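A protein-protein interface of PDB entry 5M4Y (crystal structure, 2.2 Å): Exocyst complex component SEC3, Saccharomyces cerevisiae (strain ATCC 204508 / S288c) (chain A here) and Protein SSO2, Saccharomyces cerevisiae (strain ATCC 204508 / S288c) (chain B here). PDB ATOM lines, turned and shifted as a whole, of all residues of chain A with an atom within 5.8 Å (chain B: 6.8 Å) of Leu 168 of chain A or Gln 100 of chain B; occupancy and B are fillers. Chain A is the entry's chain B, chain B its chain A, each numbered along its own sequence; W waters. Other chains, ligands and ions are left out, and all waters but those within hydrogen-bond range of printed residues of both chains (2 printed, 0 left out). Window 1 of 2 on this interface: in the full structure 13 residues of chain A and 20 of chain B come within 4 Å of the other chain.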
ATOM      1  N   ILE A 144      -0.073 -26.347 -32.214  1.00  0.00           N
ATOM      2  CA  ILE A 144       0.855 -25.778 -31.243  1.00  0.00           C
ATOM      3  C   ILE A 144       2.031 -25.113 -31.949  1.00  0.00           C
ATOM      4  O   ILE A 144       2.447 -24.011 -31.576  1.00  0.00           O
ATOM      5  CB  ILE A 144       1.315 -26.860 -30.250  1.00  0.00           C
ATOM      6  CG1 ILE A 144       0.111 -27.445 -29.509  1.00  0.00           C
ATOM      7  CG2 ILE A 144       2.317 -26.289 -29.262  1.00  0.00           C
ATOM      8  CD1 ILE A 144      -0.707 -26.413 -28.759  1.00  0.00           C
ATOM      9  N   THR A 145       2.579 -25.765 -32.979  1.00  0.00           N
ATOM     10  CA  THR A 145       3.671 -25.165 -33.741  1.00  0.00           C
ATOM     11  C   THR A 145       3.268 -23.810 -34.311  1.00  0.00           C
ATOM     12  O   THR A 145       4.039 -22.845 -34.247  1.00  0.00           O
ATOM     13  CB  THR A 145       4.116 -26.106 -34.864  1.00  0.00           C
ATOM     14  OG1 THR A 145       4.734 -27.270 -34.302  1.00  0.00           O
ATOM     15  CG2 THR A 145       5.102 -25.414 -35.785  1.00  0.00           C
ATOM     16  N   ILE A 148       3.285 -21.133 -31.368  1.00  0.00           N
ATOM     17  CA  ILE A 148       4.611 -20.650 -30.986  1.00  0.00           C
ATOM     18  C   ILE A 148       5.146 -19.687 -32.033  1.00  0.00           C
ATOM     19  O   ILE A 148       5.770 -18.669 -31.708  1.00  0.00           O
ATOM     20  CB  ILE A 148       5.574 -21.833 -30.777  1.00  0.00           C
ATOM     21  CG1 ILE A 148       4.882 -22.966 -30.023  1.00  0.00           C
ATOM     22  CG2 ILE A 148       6.819 -21.381 -30.033  1.00  0.00           C
ATOM     23  CD1 ILE A 148       5.742 -24.199 -29.830  1.00  0.00           C
ATOM     24  N   VAL A 155       3.321 -20.466 -25.690  1.00  0.00           N
ATOM     25  CA  VAL A 155       2.460 -21.638 -25.862  1.00  0.00           C
ATOM     26  C   VAL A 155       1.297 -21.549 -24.890  1.00  0.00           C
ATOM     27  O   VAL A 155       1.399 -20.956 -23.812  1.00  0.00           O
ATOM     28  CB  VAL A 155       3.224 -22.963 -25.631  1.00  0.00           C
ATOM     29  CG1 VAL A 155       4.373 -23.103 -26.598  1.00  0.00           C
ATOM     30  CG2 VAL A 155       3.735 -23.052 -24.208  1.00  0.00           C
ATOM     31  N   LEU A 158      -0.429 -26.860 -21.786  1.00  0.00           N
ATOM     32  CA  LEU A 158      -0.416 -28.188 -22.382  1.00  0.00           C
ATOM     33  C   LEU A 158      -0.586 -29.225 -21.283  1.00  0.00           C
ATOM     34  O   LEU A 158       0.156 -29.217 -20.296  1.00  0.00           O
ATOM     35  CB  LEU A 158       0.884 -28.426 -23.155  1.00  0.00           C
ATOM     36  CG  LEU A 158       1.240 -27.364 -24.200  1.00  0.00           C
ATOM     37  CD1 LEU A 158       2.533 -27.728 -24.911  1.00  0.00           C
ATOM     38  CD2 LEU A 158       0.110 -27.179 -25.201  1.00  0.00           C
ATOM     39  N   LEU A 163       6.157 -33.285 -24.559  1.00  0.00           N
ATOM     40  CA  LEU A 163       6.615 -31.960 -24.965  1.00  0.00           C
ATOM     41  C   LEU A 163       7.545 -32.024 -26.168  1.00  0.00           C
ATOM     42  O   LEU A 163       7.664 -31.043 -26.908  1.00  0.00           O
ATOM     43  CB  LEU A 163       7.303 -31.261 -23.793  1.00  0.00           C
ATOM     44  CG  LEU A 163       6.395 -30.915 -22.610  1.00  0.00           C
ATOM     45  CD1 LEU A 163       7.205 -30.337 -21.469  1.00  0.00           C
ATOM     46  CD2 LEU A 163       5.305 -29.948 -23.040  1.00  0.00           C
ATOM     47  N   SER A 164       8.208 -33.165 -26.379  1.00  0.00           N
ATOM     48  CA  SER A 164       9.085 -33.316 -27.534  1.00  0.00           C
ATOM     49  C   SER A 164       8.315 -33.320 -28.846  1.00  0.00           C
ATOM     50  O   SER A 164       8.915 -33.094 -29.902  1.00  0.00           O
ATOM     51  CB  SER A 164       9.911 -34.597 -27.407  1.00  0.00           C
ATOM     52  OG  SER A 164       9.114 -35.745 -27.619  1.00  0.00           O
ATOM     53  N   LEU A 165       7.004 -33.577 -28.806  1.00  0.00           N
ATOM     54  CA  LEU A 165       6.191 -33.477 -30.013  1.00  0.00           C
ATOM     55  C   LEU A 165       6.244 -32.076 -30.603  1.00  0.00           C
ATOM     56  O   LEU A 165       6.203 -31.914 -31.828  1.00  0.00           O
ATOM     57  CB  LEU A 165       4.745 -33.862 -29.701  1.00  0.00           C
ATOM     58  CG  LEU A 165       3.735 -33.791 -30.848  1.00  0.00           C
ATOM     59  CD1 LEU A 165       4.091 -34.795 -31.927  1.00  0.00           C
ATOM     60  CD2 LEU A 165       2.321 -34.020 -30.339  1.00  0.00           C
ATOM     61  N   PHE A 166       6.345 -31.057 -29.750  1.00  0.00           N
ATOM     62  CA  PHE A 166       6.414 -29.665 -30.169  1.00  0.00           C
ATOM     63  C   PHE A 166       7.835 -29.118 -30.112  1.00  0.00           C
ATOM     64  O   PHE A 166       8.024 -27.896 -30.118  1.00  0.00           O
ATOM     65  CB  PHE A 166       5.478 -28.819 -29.307  1.00  0.00           C
ATOM     66  CG  PHE A 166       4.170 -29.491 -29.001  1.00  0.00           C
ATOM     67  CD1 PHE A 166       3.302 -29.841 -30.023  1.00  0.00           C
ATOM     68  CD2 PHE A 166       3.811 -29.780 -27.698  1.00  0.00           C
ATOM     69  CE1 PHE A 166       2.101 -30.463 -29.749  1.00  0.00           C
ATOM     70  CE2 PHE A 166       2.612 -30.402 -27.415  1.00  0.00           C
ATOM     71  CZ  PHE A 166       1.755 -30.743 -28.440  1.00  0.00           C
ATOM     72  N   TYR A 167       8.834 -30.003 -30.062  1.00  0.00           N
ATOM     73  CA  TYR A 167      10.240 -29.616 -29.949  1.00  0.00           C
ATOM     74  C   TYR A 167      10.479 -28.770 -28.702  1.00  0.00           C
ATOM     75  O   TYR A 167      11.242 -27.802 -28.716  1.00  0.00           O
ATOM     76  CB  TYR A 167      10.724 -28.899 -31.211  1.00  0.00           C
ATOM     77  CG  TYR A 167      10.409 -29.666 -32.472  1.00  0.00           C
ATOM     78  CD1 TYR A 167      11.042 -30.869 -32.751  1.00  0.00           C
ATOM     79  CD2 TYR A 167       9.467 -29.196 -33.377  1.00  0.00           C
ATOM     80  CE1 TYR A 167      10.752 -31.581 -33.898  1.00  0.00           C
ATOM     81  CE2 TYR A 167       9.172 -29.899 -34.530  1.00  0.00           C
ATOM     82  CZ  TYR A 167       9.816 -31.091 -34.784  1.00  0.00           C
ATOM     83  OH  TYR A 167       9.525 -31.796 -35.931  1.00  0.00           O
ATOM     84  N   LEU A 168       9.813 -29.142 -27.615  1.00  0.00           N
ATOM     85  CA  LEU A 168       9.965 -28.507 -26.318  1.00  0.00           C
ATOM     86  C   LEU A 168      10.439 -29.535 -25.299  1.00  0.00           C
ATOM     87  O   LEU A 168      10.329 -30.745 -25.506  1.00  0.00           O
ATOM     88  CB  LEU A 168       8.644 -27.889 -25.837  1.00  0.00           C
ATOM     89  CG  LEU A 168       7.985 -26.782 -26.661  1.00  0.00           C
ATOM     90  CD1 LEU A 168       6.576 -26.521 -26.155  1.00  0.00           C
ATOM     91  CD2 LEU A 168       8.812 -25.514 -26.597  1.00  0.00           C
ATOM     92  N   ASP A 169      10.975 -29.034 -24.190  1.00  0.00           N
ATOM     93  CA  ASP A 169      11.172 -29.830 -22.989  1.00  0.00           C
ATOM     94  C   ASP A 169      10.522 -29.093 -21.823  1.00  0.00           C
ATOM     95  O   ASP A 169       9.948 -28.012 -21.991  1.00  0.00           O
ATOM     96  CB  ASP A 169      12.658 -30.120 -22.727  1.00  0.00           C
ATOM     97  CG  ASP A 169      13.509 -28.861 -22.620  1.00  0.00           C
ATOM     98  OD1 ASP A 169      12.957 -27.751 -22.483  1.00  0.00           O
ATOM     99  OD2 ASP A 169      14.750 -28.990 -22.663  1.00  0.00           O
ATOM    100  N   GLU A 170      10.607 -29.688 -20.632  1.00  0.00           N
ATOM    101  CA  GLU A 170      10.021 -29.056 -19.455  1.00  0.00           C
ATOM    102  C   GLU A 170      10.627 -27.681 -19.208  1.00  0.00           C
ATOM    103  O   GLU A 170       9.924 -26.747 -18.802  1.00  0.00           O
ATOM    104  CB  GLU A 170      10.206 -29.954 -18.232  1.00  0.00           C
ATOM    105  CG  GLU A 170       9.538 -29.432 -16.969  1.00  0.00           C
ATOM    106  CD  GLU A 170       8.023 -29.423 -17.069  1.00  0.00           C
ATOM    107  OE1 GLU A 170       7.470 -30.228 -17.847  1.00  0.00           O
ATOM    108  OE2 GLU A 170       7.385 -28.610 -16.368  1.00  0.00           O
ATOM    109  N   SER A 172      12.030 -25.444 -21.456  1.00  0.00           N
ATOM    110  CA  SER A 172      11.570 -24.452 -22.420  1.00  0.00           C
ATOM    111  C   SER A 172      10.061 -24.249 -22.371  1.00  0.00           C
ATOM    112  O   SER A 172       9.574 -23.178 -22.747  1.00  0.00           O
ATOM    113  CB  SER A 172      11.997 -24.851 -23.834  1.00  0.00           C
ATOM    114  OG  SER A 172      11.438 -26.097 -24.207  1.00  0.00           O
ATOM    115  N   TYR A 173       9.305 -25.254 -21.922  1.00  0.00           N
ATOM    116  CA  TYR A 173       7.861 -25.085 -21.795  1.00  0.00           C
ATOM    117  C   TYR A 173       7.523 -24.075 -20.710  1.00  0.00           C
ATOM    118  O   TYR A 173       6.663 -23.208 -20.900  1.00  0.00           O
ATOM    119  CB  TYR A 173       7.191 -26.427 -21.505  1.00  0.00           C
ATOM    120  CG  TYR A 173       5.737 -26.309 -21.093  1.00  0.00           C
ATOM    121  CD1 TYR A 173       4.749 -26.046 -22.034  1.00  0.00           C
ATOM    122  CD2 TYR A 173       5.352 -26.458 -19.766  1.00  0.00           C
ATOM    123  CE1 TYR A 173       3.421 -25.934 -21.664  1.00  0.00           C
ATOM    124  CE2 TYR A 173       4.026 -26.348 -19.387  1.00  0.00           C
ATOM    125  CZ  TYR A 173       3.066 -26.086 -20.341  1.00  0.00           C
ATOM    126  OH  TYR A 173       1.746 -25.975 -19.972  1.00  0.00           O
ATOM    127  N   ALA A 176       8.020 -20.548 -21.736  1.00  0.00           N
ATOM    128  CA  ALA A 176       7.199 -20.092 -22.847  1.00  0.00           C
ATOM    129  C   ALA A 176       5.706 -20.066 -22.559  1.00  0.00           C
ATOM    130  O   ALA A 176       4.983 -19.337 -23.242  1.00  0.00           O
ATOM    131  CB  ALA A 176       7.440 -20.974 -24.081  1.00  0.00           C
ATOM    132  N   TYR B  23      26.216 -25.655 -31.203  1.00  0.00           N
ATOM    133  CA  TYR B  23      25.092 -24.736 -31.346  1.00  0.00           C
ATOM    134  C   TYR B  23      24.368 -24.536 -30.020  1.00  0.00           C
ATOM    135  O   TYR B  23      23.954 -23.418 -29.697  1.00  0.00           O
ATOM    136  CB  TYR B  23      24.140 -25.268 -32.419  1.00  0.00           C
ATOM    137  CG  TYR B  23      22.951 -24.393 -32.747  1.00  0.00           C
ATOM    138  CD1 TYR B  23      23.114 -23.056 -33.088  1.00  0.00           C
ATOM    139  CD2 TYR B  23      21.665 -24.918 -32.760  1.00  0.00           C
ATOM    140  CE1 TYR B  23      22.025 -22.263 -33.405  1.00  0.00           C
ATOM    141  CE2 TYR B  23      20.574 -24.138 -33.076  1.00  0.00           C
ATOM    142  CZ  TYR B  23      20.759 -22.811 -33.398  1.00  0.00           C
ATOM    143  OH  TYR B  23      19.670 -22.032 -33.713  1.00  0.00           O
ATOM    144  N   ILE B  27      23.773 -20.938 -27.893  1.00  0.00           N
ATOM    145  CA  ILE B  27      22.441 -20.463 -27.524  1.00  0.00           C
ATOM    146  C   ILE B  27      22.388 -20.107 -26.044  1.00  0.00           C
ATOM    147  O   ILE B  27      21.767 -19.112 -25.650  1.00  0.00           O
ATOM    148  CB  ILE B  27      21.382 -21.517 -27.897  1.00  0.00           C
ATOM    149  CG1 ILE B  27      21.297 -21.668 -29.414  1.00  0.00           C
ATOM    150  CG2 ILE B  27      20.026 -21.150 -27.321  1.00  0.00           C
ATOM    151  CD1 ILE B  27      20.338 -22.746 -29.861  1.00  0.00           C
ATOM    152  N   PHE B  95      18.056 -30.669 -33.842  1.00  0.00           N
ATOM    153  CA  PHE B  95      18.259 -29.329 -34.384  1.00  0.00           C
ATOM    154  C   PHE B  95      17.031 -28.459 -34.152  1.00  0.00           C
ATOM    155  O   PHE B  95      17.144 -27.305 -33.725  1.00  0.00           O
ATOM    156  CB  PHE B  95      18.589 -29.423 -35.876  1.00  0.00           C
ATOM    157  CG  PHE B  95      18.972 -28.110 -36.508  1.00  0.00           C
ATOM    158  CD1 PHE B  95      19.524 -27.088 -35.756  1.00  0.00           C
ATOM    159  CD2 PHE B  95      18.777 -27.903 -37.866  1.00  0.00           C
ATOM    160  CE1 PHE B  95      19.873 -25.886 -36.344  1.00  0.00           C
ATOM    161  CE2 PHE B  95      19.124 -26.705 -38.458  1.00  0.00           C
ATOM    162  CZ  PHE B  95      19.673 -25.695 -37.696  1.00  0.00           C
ATOM    163  N   LEU B  96      15.841 -29.008 -34.411  1.00  0.00           N
ATOM    164  CA  LEU B  96      14.614 -28.233 -34.263  1.00  0.00           C
ATOM    165  C   LEU B  96      14.360 -27.859 -32.809  1.00  0.00           C
ATOM    166  O   LEU B  96      13.844 -26.773 -32.525  1.00  0.00           O
ATOM    167  CB  LEU B  96      13.432 -29.016 -34.834  1.00  0.00           C
ATOM    168  CG  LEU B  96      13.416 -29.157 -36.357  1.00  0.00           C
ATOM    169  CD1 LEU B  96      12.509 -30.295 -36.790  1.00  0.00           C
ATOM    170  CD2 LEU B  96      12.977 -27.855 -37.003  1.00  0.00           C
ATOM    171  N   LYS B  97      14.712 -28.745 -31.875  1.00  0.00           N
ATOM    172  CA  LYS B  97      14.516 -28.444 -30.460  1.00  0.00           C
ATOM    173  C   LYS B  97      15.395 -27.280 -30.022  1.00  0.00           C
ATOM    174  O   LYS B  97      14.986 -26.457 -29.194  1.00  0.00           O
ATOM    175  CB  LYS B  97      14.802 -29.690 -29.618  1.00  0.00           C
ATOM    176  CG  LYS B  97      14.455 -29.560 -28.138  1.00  0.00           C
ATOM    177  CD  LYS B  97      15.660 -29.152 -27.302  1.00  0.00           C
ATOM    178  CE  LYS B  97      15.272 -28.928 -25.852  1.00  0.00           C
ATOM    179  NZ  LYS B  97      16.423 -28.435 -25.046  1.00  0.00           N
ATOM    180  N   LEU B  98      16.608 -27.196 -30.570  1.00  0.00           N
ATOM    181  CA  LEU B  98      17.503 -26.097 -30.226  1.00  0.00           C
ATOM    182  C   LEU B  98      17.049 -24.794 -30.871  1.00  0.00           C
ATOM    183  O   LEU B  98      17.150 -23.724 -30.258  1.00  0.00           O
ATOM    184  CB  LEU B  98      18.933 -26.442 -30.640  1.00  0.00           C
ATOM    185  CG  LEU B  98      19.546 -27.641 -29.914  1.00  0.00           C
ATOM    186  CD1 LEU B  98      20.891 -28.013 -30.519  1.00  0.00           C
ATOM    187  CD2 LEU B  98      19.686 -27.346 -28.429  1.00  0.00           C
ATOM    188  N   ILE B  99      16.553 -24.863 -32.109  1.00  0.00           N
ATOM    189  CA  ILE B  99      15.949 -23.691 -32.735  1.00  0.00           C
ATOM    190  C   ILE B  99      14.784 -23.190 -31.893  1.00  0.00           C
ATOM    191  O   ILE B  99      14.583 -21.980 -31.737  1.00  0.00           O
ATOM    192  CB  ILE B  99      15.509 -24.017 -34.175  1.00  0.00           C
ATOM    193  CG1 ILE B  99      16.714 -24.430 -35.023  1.00  0.00           C
ATOM    194  CG2 ILE B  99      14.800 -22.828 -34.806  1.00  0.00           C
ATOM    195  CD1 ILE B  99      16.340 -25.003 -36.371  1.00  0.00           C
ATOM    196  N   GLN B 100      14.005 -24.115 -31.328  1.00  0.00           N
ATOM    197  CA  GLN B 100      12.904 -23.727 -30.454  1.00  0.00           C
ATOM    198  C   GLN B 100      13.423 -23.084 -29.174  1.00  0.00           C
ATOM    199  O   GLN B 100      12.830 -22.124 -28.668  1.00  0.00           O
ATOM    200  CB  GLN B 100      12.041 -24.947 -30.136  1.00  0.00           C
ATOM    201  CG  GLN B 100      10.632 -24.622 -29.660  1.00  0.00           C
ATOM    202  CD  GLN B 100       9.728 -24.158 -30.785  1.00  0.00           C
ATOM    203  OE1 GLN B 100       9.860 -23.040 -31.283  1.00  0.00           O
ATOM    204  NE2 GLN B 100       8.802 -25.016 -31.192  1.00  0.00           N
ATOM    205  N   ASP B 101      14.531 -23.601 -28.637  1.00  0.00           N
ATOM    206  CA  ASP B 101      15.156 -22.982 -27.472  1.00  0.00           C
ATOM    207  C   ASP B 101      15.598 -21.558 -27.784  1.00  0.00           C
ATOM    208  O   ASP B 101      15.315 -20.626 -27.023  1.00  0.00           O
ATOM    209  CB  ASP B 101      16.344 -23.826 -27.005  1.00  0.00           C
ATOM    210  CG  ASP B 101      15.917 -25.115 -26.333  1.00  0.00           C
ATOM    211  OD1 ASP B 101      14.728 -25.226 -25.968  1.00  0.00           O
ATOM    212  OD2 ASP B 101      16.770 -26.012 -26.158  1.00  0.00           O
ATOM    213  N   TYR B 102      16.295 -21.374 -28.908  1.00  0.00           N
ATOM    214  CA  TYR B 102      16.765 -20.048 -29.299  1.00  0.00           C
ATOM    215  C   TYR B 102      15.599 -19.077 -29.447  1.00  0.00           C
ATOM    216  O   TYR B 102      15.648 -17.947 -28.949  1.00  0.00           O
ATOM    217  CB  TYR B 102      17.561 -20.153 -30.602  1.00  0.00           C
ATOM    218  CG  TYR B 102      18.357 -18.922 -30.988  1.00  0.00           C
ATOM    219  CD1 TYR B 102      18.411 -17.807 -30.163  1.00  0.00           C
ATOM    220  CD2 TYR B 102      19.052 -18.878 -32.190  1.00  0.00           C
ATOM    221  CE1 TYR B 102      19.132 -16.687 -30.520  1.00  0.00           C
ATOM    222  CE2 TYR B 102      19.777 -17.761 -32.555  1.00  0.00           C
ATOM    223  CZ  TYR B 102      19.814 -16.669 -31.717  1.00  0.00           C
ATOM    224  OH  TYR B 102      20.536 -15.556 -32.078  1.00  0.00           O
ATOM    225  N   ARG B 103      14.535 -19.511 -30.126  1.00  0.00           N
ATOM    226  CA  ARG B 103      13.362 -18.662 -30.300  1.00  0.00           C
ATOM    227  C   ARG B 103      12.786 -18.232 -28.957  1.00  0.00           C
ATOM    228  O   ARG B 103      12.464 -17.057 -28.754  1.00  0.00           O
ATOM    229  CB  ARG B 103      12.309 -19.399 -31.128  1.00  0.00           C
ATOM    230  CG  ARG B 103      10.895 -18.870 -30.962  1.00  0.00           C
ATOM    231  CD  ARG B 103       9.886 -19.788 -31.639  1.00  0.00           C
ATOM    232  NE  ARG B 103       9.899 -19.662 -33.093  1.00  0.00           N
ATOM    233  CZ  ARG B 103       9.378 -20.558 -33.927  1.00  0.00           C
ATOM    234  NH1 ARG B 103       8.811 -21.659 -33.452  1.00  0.00           N
ATOM    235  NH2 ARG B 103       9.433 -20.356 -35.235  1.00  0.00           N
ATOM    236  N   ILE B 104      12.658 -19.174 -28.023  1.00  0.00           N
ATOM    237  CA  ILE B 104      12.084 -18.854 -26.720  1.00  0.00           C
ATOM    238  C   ILE B 104      13.026 -17.958 -25.925  1.00  0.00           C
ATOM    239  O   ILE B 104      12.585 -17.066 -25.191  1.00  0.00           O
ATOM    240  CB  ILE B 104      11.745 -20.150 -25.960  1.00  0.00           C
ATOM    241  CG1 ILE B 104      10.648 -20.924 -26.693  1.00  0.00           C
ATOM    242  CG2 ILE B 104      11.313 -19.848 -24.531  1.00  0.00           C
ATOM    243  CD1 ILE B 104      10.332 -22.263 -26.067  1.00  0.00           C
ATOM    244  N   ILE B 105      14.334 -18.170 -26.067  1.00  0.00           N
ATOM    245  CA  ILE B 105      15.303 -17.346 -25.352  1.00  0.00           C
ATOM    246  C   ILE B 105      15.242 -15.903 -25.837  1.00  0.00           C
ATOM    247  O   ILE B 105      15.241 -14.963 -25.033  1.00  0.00           O
ATOM    248  CB  ILE B 105      16.714 -17.949 -25.490  1.00  0.00           C
ATOM    249  CG1 ILE B 105      16.959 -18.957 -24.366  1.00  0.00           C
ATOM    250  CG2 ILE B 105      17.779 -16.863 -25.507  1.00  0.00           C
ATOM    251  CD1 ILE B 105      18.185 -19.812 -24.560  1.00  0.00           C
ATOM    252  N   PHE B 187      12.976 -22.893 -39.243  1.00  0.00           N
ATOM    253  CA  PHE B 187      12.147 -23.941 -38.657  1.00  0.00           C
ATOM    254  C   PHE B 187      11.253 -24.589 -39.707  1.00  0.00           C
ATOM    255  O   PHE B 187      11.107 -25.817 -39.739  1.00  0.00           O
ATOM    256  CB  PHE B 187      11.311 -23.353 -37.519  1.00  0.00           C
ATOM    257  CG  PHE B 187      10.582 -24.375 -36.700  1.00  0.00           C
ATOM    258  CD1 PHE B 187      11.216 -25.025 -35.656  1.00  0.00           C
ATOM    259  CD2 PHE B 187       9.254 -24.670 -36.958  1.00  0.00           C
ATOM    260  CE1 PHE B 187      10.545 -25.960 -34.895  1.00  0.00           C
ATOM    261  CE2 PHE B 187       8.578 -25.603 -36.200  1.00  0.00           C
ATOM    262  CZ  PHE B 187       9.223 -26.248 -35.167  1.00  0.00           C
HETATM  263  O   HOH W   1      15.083 -26.225 -22.915  1.00  0.00           O
HETATM  264  O   HOH W   2      12.407 -25.976 -26.777  1.00  0.00           O
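Water W2 lies within hydrogen-bond range of the side-chain carboxylate (OD1) of Asp 101 of chain B (2.6 Å), the side-chain hydroxyl (OG) of Ser 172 of chain A (2.7 Å) and the backbone carbonyl oxygen (O) of Tyr 167 of chain A (2.9 Å).
Water W1 lies within hydrogen-bond range of OD1 of Asp 169 of chain A (2.7 Å), OD1 of Asp 101 of chain B (3.2 Å), NZ of Lys 97 of chain B (3.3 Å) and N of Ser 172 of chain A (3.5 Å).
NZ of Lys 97 of chain B is in salt-bridge range of OD2 of Asp 101 of chain B (2.7 Å).
The side-chain amide oxygen (OE1) of Gln 100 of chain B is in hydrogen-bond range of the guanidinium group (NH1) of Arg 103 of chain B.
O of Ala 176 of chain A is in hydrogen-bond range of N of Val 155 of chain A (3.2 Å).
The backbone carbonyl oxygen (O) of Leu 163 of chain A sits at hydrogen-bond distance from the backbone NH (N) of Leu 168 of chain A (3.0 Å).
OD1 of Asp 169 of chain A lies within hydrogen-bond range of N of Ser 172 of chain A (2.7 Å).
Of chain B, only Gln 100 (3.7 Å) and Ile 104 (3.6 Å) come within 4 Å of Leu 168 of chain A.
Gln 100 of chain B touches just these residues of chain A: Ile 148 (3.4 Å), Phe 166 (3.2 Å), Tyr 167 (3.3 Å) and Leu 168 (3.7 Å).
Of the printed residues of chain B, Thr 145 of chain A touches Phe 187 (3.5 Å).
Of the printed residues of chain A, Phe 187 of chain B touches Thr 145 (3.5 Å) and Tyr 167 (3.5 Å).
Of the printed residues of chain B, Ile 148 of chain A touches Gln 100 and Arg 103.
Of the printed residues of chain A, Leu 96 of chain B touches Tyr 167.
Of the printed residues of chain B, Ala 176 of chain A touches Ile 104.
Leu 98 of chain B touches none of the printed residues of chain A.
The nearest residue of chain B that does not touch Leu 168 of chain A is Lys 97 of chain B (4.7 Å).
Printed residues of chain B that touch a printed residue of chain A: Leu 96, Lys 97, Gln 100, Asp 101, Arg 103, Ile 104 and Phe 187.
Hydrophobic or aromatic side chains of chain A that line the printed part of chain B: Ile 148, Tyr 167, Leu 168 and Ala 176.
Among the printed residues, 14 pairs touch across the chains.
Among the printed residues, Asp or Glu carboxylates within 4 Å of a Lys or Arg side-chain nitrogen of the other chain: Asp 169 of chain A with Lys 97 of chain B.
The side-chain amino group of Lys 97 of chain B lies within salt-bridge range of the side-chain carboxylate of Asp 169 of chain A, 3.0 Å away.
The side-chain amide nitrogen (NE2) of Gln 100 of chain B is in hydrogen-bond range of the backbone carbonyl oxygen (O) of Phe 166 of chain A (3.2 Å).
Among the printed residues, merely in contact across the chains: Thr 145 of chain A with Phe 187 of chain B, Ile 148 of chain A with Gln 100 of chain B, Ile 148 of chain A with Arg 103 of chain B, Tyr 167 of chain A with Leu 96 of chain B, Tyr 167 of chain A with Lys 97 of chain B, Tyr 167 of chain A with Gln 100 of chain B, Tyr 167 of chain A with Phe 187 of chain B, Leu 168 of chain A with Gln 100 of chain B, Leu 168 of chain A with Ile 104 of chain B, Ser 172 of chain A with Asp 101 of chain B, Ser 172 of chain A with Ile 104 of chain B and Ala 176 of chain A with Ile 104 of chain B.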
